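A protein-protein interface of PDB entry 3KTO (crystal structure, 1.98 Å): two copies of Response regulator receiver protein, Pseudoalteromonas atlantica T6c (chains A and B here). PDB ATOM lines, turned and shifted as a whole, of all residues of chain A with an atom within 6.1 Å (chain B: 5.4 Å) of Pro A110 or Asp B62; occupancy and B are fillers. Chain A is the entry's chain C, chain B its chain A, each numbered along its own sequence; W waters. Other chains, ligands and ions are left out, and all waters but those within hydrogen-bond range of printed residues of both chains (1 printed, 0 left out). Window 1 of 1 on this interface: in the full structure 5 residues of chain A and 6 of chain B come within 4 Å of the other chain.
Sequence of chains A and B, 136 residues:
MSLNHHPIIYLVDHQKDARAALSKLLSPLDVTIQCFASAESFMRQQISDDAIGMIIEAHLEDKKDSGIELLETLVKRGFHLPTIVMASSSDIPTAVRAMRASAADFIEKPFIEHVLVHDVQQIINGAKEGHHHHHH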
ATOM      1  N   ALA A  18      27.316 -32.016 -11.210  1.00  0.00           N
ATOM      2  CA  ALA A  18      27.584 -30.877 -12.080  1.00  0.00           C
ATOM      3  C   ALA A  18      27.526 -31.307 -13.541  1.00  0.00           C
ATOM      4  O   ALA A  18      26.924 -30.628 -14.371  1.00  0.00           O
ATOM      5  CB  ALA A  18      28.953 -30.284 -11.760  1.00  0.00           C
ATOM      6  N   LEU A  22      24.834 -29.545 -16.134  1.00  0.00           N
ATOM      7  CA  LEU A  22      25.286 -28.839 -17.326  1.00  0.00           C
ATOM      8  C   LEU A  22      24.770 -29.531 -18.575  1.00  0.00           C
ATOM      9  O   LEU A  22      24.337 -28.870 -19.519  1.00  0.00           O
ATOM     10  CB  LEU A  22      26.812 -28.758 -17.370  1.00  0.00           C
ATOM     11  CG  LEU A  22      27.447 -27.651 -16.529  1.00  0.00           C
ATOM     12  CD1 LEU A  22      27.022 -27.792 -15.082  1.00  0.00           C
ATOM     13  CD2 LEU A  22      28.961 -27.731 -16.654  1.00  0.00           C
ATOM     14  N   ALA A  87      35.070 -22.203 -13.352  1.00  0.00           N
ATOM     15  CA  ALA A  87      35.669 -22.393 -12.041  1.00  0.00           C
ATOM     16  C   ALA A  87      34.820 -21.764 -10.953  1.00  0.00           C
ATOM     17  O   ALA A  87      34.247 -20.691 -11.135  1.00  0.00           O
ATOM     18  CB  ALA A  87      37.078 -21.800 -12.024  1.00  0.00           C
ATOM     19  N   SER A  88      34.730 -22.439  -9.819  1.00  0.00           N
ATOM     20  CA  SER A  88      33.954 -21.910  -8.710  1.00  0.00           C
ATOM     21  C   SER A  88      34.913 -21.093  -7.862  1.00  0.00           C
ATOM     22  O   SER A  88      34.664 -19.924  -7.554  1.00  0.00           O
ATOM     23  CB  SER A  88      33.339 -23.051  -7.902  1.00  0.00           C
ATOM     24  OG  SER A  88      34.341 -23.919  -7.421  1.00  0.00           O
ATOM     25  N   GLU A 108      32.784 -17.987 -14.084  1.00  0.00           N
ATOM     26  CA  GLU A 108      32.801 -18.282 -12.660  1.00  0.00           C
ATOM     27  C   GLU A 108      31.531 -19.045 -12.323  1.00  0.00           C
ATOM     28  O   GLU A 108      30.475 -18.790 -12.902  1.00  0.00           O
ATOM     29  CB  GLU A 108      32.796 -16.998 -11.840  1.00  0.00           C
ATOM     30  CG  GLU A 108      33.953 -16.067 -12.051  1.00  0.00           C
ATOM     31  CD  GLU A 108      33.674 -14.717 -11.425  1.00  0.00           C
ATOM     32  OE1 GLU A 108      32.972 -13.895 -12.052  1.00  0.00           O
ATOM     33  OE2 GLU A 108      34.133 -14.493 -10.291  1.00  0.00           O
ATOM     34  N   LYS A 109      31.639 -19.988 -11.396  1.00  0.00           N
ATOM     35  CA  LYS A 109      30.484 -20.749 -10.935  1.00  0.00           C
ATOM     36  C   LYS A 109      30.351 -20.369  -9.470  1.00  0.00           C
ATOM     37  O   LYS A 109      31.357 -20.137  -8.804  1.00  0.00           O
ATOM     38  CB  LYS A 109      30.728 -22.256 -11.038  1.00  0.00           C
ATOM     39  CG  LYS A 109      30.800 -22.768 -12.452  1.00  0.00           C
ATOM     40  CD  LYS A 109      30.946 -24.264 -12.481  1.00  0.00           C
ATOM     41  CE  LYS A 109      32.308 -24.697 -11.991  1.00  0.00           C
ATOM     42  NZ  LYS A 109      32.531 -26.126 -12.329  1.00  0.00           N
ATOM     43  N   PRO A 110      29.115 -20.262  -8.951  1.00  0.00           N
ATOM     44  CA  PRO A 110      27.837 -20.471  -9.640  1.00  0.00           C
ATOM     45  C   PRO A 110      27.721 -19.541 -10.844  1.00  0.00           C
ATOM     46  O   PRO A 110      28.038 -18.355 -10.765  1.00  0.00           O
ATOM     47  CB  PRO A 110      26.805 -20.173  -8.556  1.00  0.00           C
ATOM     48  CG  PRO A 110      27.512 -19.205  -7.668  1.00  0.00           C
ATOM     49  CD  PRO A 110      28.893 -19.803  -7.572  1.00  0.00           C
ATOM     50  N   PHE A 111      27.245 -20.098 -11.947  1.00  0.00           N
ATOM     51  CA  PHE A 111      27.143 -19.370 -13.200  1.00  0.00           C
ATOM     52  C   PHE A 111      25.770 -18.843 -13.598  1.00  0.00           C
ATOM     53  O   PHE A 111      24.734 -19.265 -13.075  1.00  0.00           O
ATOM     54  CB  PHE A 111      27.671 -20.259 -14.328  1.00  0.00           C
ATOM     55  CG  PHE A 111      26.893 -21.542 -14.501  1.00  0.00           C
ATOM     56  CD1 PHE A 111      27.087 -22.613 -13.639  1.00  0.00           C
ATOM     57  CD2 PHE A 111      25.956 -21.667 -15.520  1.00  0.00           C
ATOM     58  CE1 PHE A 111      26.365 -23.795 -13.792  1.00  0.00           C
ATOM     59  CE2 PHE A 111      25.225 -22.844 -15.684  1.00  0.00           C
ATOM     60  CZ  PHE A 111      25.428 -23.909 -14.818  1.00  0.00           C
ATOM     61  N   ILE A 112      25.791 -17.898 -14.536  1.00  0.00           N
ATOM     62  CA  ILE A 112      24.582 -17.305 -15.074  1.00  0.00           C
ATOM     63  C   ILE A 112      24.254 -18.175 -16.279  1.00  0.00           C
ATOM     64  O   ILE A 112      25.050 -18.302 -17.208  1.00  0.00           O
ATOM     65  CB  ILE A 112      24.802 -15.842 -15.538  1.00  0.00           C
ATOM     66  CG1 ILE A 112      25.149 -14.940 -14.347  1.00  0.00           C
ATOM     67  CG2 ILE A 112      23.539 -15.323 -16.213  1.00  0.00           C
ATOM     68  CD1 ILE A 112      26.542 -15.141 -13.779  1.00  0.00           C
ATOM     69  N   HIS B  14      20.663 -28.205  -2.911  1.00  0.00           N
ATOM     70  CA  HIS B  14      21.061 -29.320  -3.770  1.00  0.00           C
ATOM     71  C   HIS B  14      22.230 -30.143  -3.218  1.00  0.00           C
ATOM     72  O   HIS B  14      22.579 -31.185  -3.773  1.00  0.00           O
ATOM     73  CB  HIS B  14      21.440 -28.801  -5.152  1.00  0.00           C
ATOM     74  CG  HIS B  14      22.619 -27.882  -5.138  1.00  0.00           C
ATOM     75  ND1 HIS B  14      22.572 -26.628  -4.575  1.00  0.00           N
ATOM     76  CD2 HIS B  14      23.893 -28.058  -5.560  1.00  0.00           C
ATOM     77  CE1 HIS B  14      23.768 -26.068  -4.651  1.00  0.00           C
ATOM     78  NE2 HIS B  14      24.587 -26.916  -5.244  1.00  0.00           N
ATOM     79  N   HIS B  59      22.349 -20.476  -4.490  1.00  0.00           N
ATOM     80  CA  HIS B  59      22.736 -20.923  -5.827  1.00  0.00           C
ATOM     81  C   HIS B  59      22.438 -22.396  -6.091  1.00  0.00           C
ATOM     82  O   HIS B  59      23.353 -23.197  -6.304  1.00  0.00           O
ATOM     83  CB  HIS B  59      24.226 -20.654  -6.024  1.00  0.00           C
ATOM     84  CG  HIS B  59      24.647 -19.282  -5.601  1.00  0.00           C
ATOM     85  ND1 HIS B  59      24.028 -18.139  -6.058  1.00  0.00           N
ATOM     86  CD2 HIS B  59      25.625 -18.870  -4.760  1.00  0.00           C
ATOM     87  CE1 HIS B  59      24.607 -17.081  -5.518  1.00  0.00           C
ATOM     88  NE2 HIS B  59      25.580 -17.498  -4.725  1.00  0.00           N
ATOM     89  N   LEU B  60      21.155 -22.738  -6.070  1.00  0.00           N
ATOM     90  CA  LEU B  60      20.723 -24.110  -6.297  1.00  0.00           C
ATOM     91  C   LEU B  60      21.286 -24.673  -7.597  1.00  0.00           C
ATOM     92  O   LEU B  60      21.222 -24.031  -8.645  1.00  0.00           O
ATOM     93  CB  LEU B  60      19.194 -24.178  -6.299  1.00  0.00           C
ATOM     94  CG  LEU B  60      18.563 -23.899  -4.933  1.00  0.00           C
ATOM     95  CD1 LEU B  60      17.073 -23.629  -5.094  1.00  0.00           C
ATOM     96  CD2 LEU B  60      18.806 -25.077  -3.999  1.00  0.00           C
ATOM     97  N   GLU B  61      21.858 -25.868  -7.501  1.00  0.00           N
ATOM     98  CA  GLU B  61      22.460 -26.560  -8.634  1.00  0.00           C
ATOM     99  C   GLU B  61      23.516 -25.736  -9.372  1.00  0.00           C
ATOM    100  O   GLU B  61      23.760 -25.934 -10.559  1.00  0.00           O
ATOM    101  CB  GLU B  61      21.369 -27.033  -9.601  1.00  0.00           C
ATOM    102  CG  GLU B  61      20.343 -27.923  -8.911  1.00  0.00           C
ATOM    103  CD  GLU B  61      19.538 -28.781  -9.869  1.00  0.00           C
ATOM    104  OE1 GLU B  61      18.966 -28.238 -10.836  1.00  0.00           O
ATOM    105  OE2 GLU B  61      19.470 -30.007  -9.643  1.00  0.00           O
ATOM    106  N   ASP B  62      24.160 -24.825  -8.651  1.00  0.00           N
ATOM    107  CA  ASP B  62      25.201 -23.988  -9.235  1.00  0.00           C
ATOM    108  C   ASP B  62      24.679 -22.940 -10.223  1.00  0.00           C
ATOM    109  O   ASP B  62      25.451 -22.365 -10.995  1.00  0.00           O
ATOM    110  CB  ASP B  62      26.264 -24.870  -9.894  1.00  0.00           C
ATOM    111  CG  ASP B  62      27.664 -24.580  -9.376  1.00  0.00           C
ATOM    112  OD1 ASP B  62      27.791 -24.059  -8.246  1.00  0.00           O
ATOM    113  OD2 ASP B  62      28.638 -24.885 -10.096  1.00  0.00           O
ATOM    114  N   LYS B  63      23.367 -22.707 -10.190  1.00  0.00           N
ATOM    115  CA  LYS B  63      22.721 -21.690 -11.020  1.00  0.00           C
ATOM    116  C   LYS B  63      22.681 -20.448 -10.132  1.00  0.00           C
ATOM    117  O   LYS B  63      21.895 -20.372  -9.197  1.00  0.00           O
ATOM    118  CB  LYS B  63      21.298 -22.107 -11.395  1.00  0.00           C
ATOM    119  CG  LYS B  63      21.223 -23.093 -12.549  1.00  0.00           C
ATOM    120  CD  LYS B  63      21.796 -24.447 -12.198  1.00  0.00           C
ATOM    121  CE  LYS B  63      21.824 -25.359 -13.424  1.00  0.00           C
ATOM    122  NZ  LYS B  63      20.525 -25.346 -14.151  1.00  0.00           N
ATOM    123  N   LYS B  64      23.541 -19.481 -10.426  1.00  0.00           N
ATOM    124  CA  LYS B  64      23.642 -18.283  -9.614  1.00  0.00           C
ATOM    125  C   LYS B  64      22.310 -17.642  -9.292  1.00  0.00           C
ATOM    126  O   LYS B  64      21.497 -17.412 -10.173  1.00  0.00           O
ATOM    127  CB  LYS B  64      24.553 -17.253 -10.285  1.00  0.00           C
ATOM    128  CG  LYS B  64      24.955 -16.120  -9.349  1.00  0.00           C
ATOM    129  CD  LYS B  64      25.903 -15.159 -10.044  1.00  0.00           C
ATOM    130  CE  LYS B  64      26.480 -14.147  -9.067  1.00  0.00           C
ATOM    131  NZ  LYS B  64      27.330 -13.144  -9.770  1.00  0.00           N
ATOM    132  N   SER B  89      29.081 -19.487  -1.570  1.00  0.00           N
ATOM    133  CA  SER B  89      29.695 -18.593  -2.538  1.00  0.00           C
ATOM    134  C   SER B  89      28.804 -17.366  -2.648  1.00  0.00           C
ATOM    135  O   SER B  89      27.590 -17.488  -2.834  1.00  0.00           O
ATOM    136  CB  SER B  89      29.785 -19.277  -3.900  1.00  0.00           C
ATOM    137  OG  SER B  89      30.222 -18.368  -4.893  1.00  0.00           O
HETATM  138  O   HOH W   1      32.247 -19.519  -6.206  1.00  0.00           O
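Among the printed residues, merely in contact across the chains: Pro A110 with Ser B89, Pro A110 with Asp B62, Lys A109 with Asp B62, Pro A110 with His B59, Pro A110 with Lys B64, Phe A111 with Lys B63 and Ile A112 with Lys B64.
The backbone carbonyl oxygen (O) of Asp B62 sits at hydrogen-bond distance from the backbone NH (N) of Phe A111, at 3.0 Å. N of Lys B64 sits at hydrogen-bond distance from O of Phe A111 (2.9 Å).
The backbone carbonyl oxygen (O) of Ser B89 is in hydrogen-bond range of a ring nitrogen (NE2) of His B59 (2.8 Å). The backbone NH of Lys A109 sits at hydrogen-bond distance from the backbone carbonyl oxygen of Ala A87, at 2.7 Å.
Water W1 lies within hydrogen-bond range of OG of Ser B89, O of Ser A88 and O of Lys A109.
No position is printed for both chains.
Ala A18 touches none of the printed residues of chain B. Printed residues of chain B within 4 Å of Lys A109: Asp B62. Of chain A, only Lys A109, Pro A110 and Phe A111 come within 4 Å of Asp B62. Of the printed residues of chain A, Lys B63 touches Phe A111. Of the printed residues of chain A, Ser B89 touches Pro A110 (3.3 Å). The nearest residue of chain A that does not touch Asp B62 is Ser A88 (5.5 Å). The nearest printed residue of chain A that does not touch His B59 is Phe A111 (6.7 Å).
Of the 9 printed residues of chain A, 4 touch a printed residue of chain B. Printed residues of chain A that touch a printed residue of chain B: Lys A109, Pro A110, Phe A111 and Ile A112. Hydrophobic or aromatic side chains of chain B that line the printed part of chain A: His B59. Among the printed residues, 9 pairs touch across the chains. Among the printed residues, no Asp or Glu carboxylate lies within 4 Å of a Lys or Arg side-chain nitrogen of the other chain.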
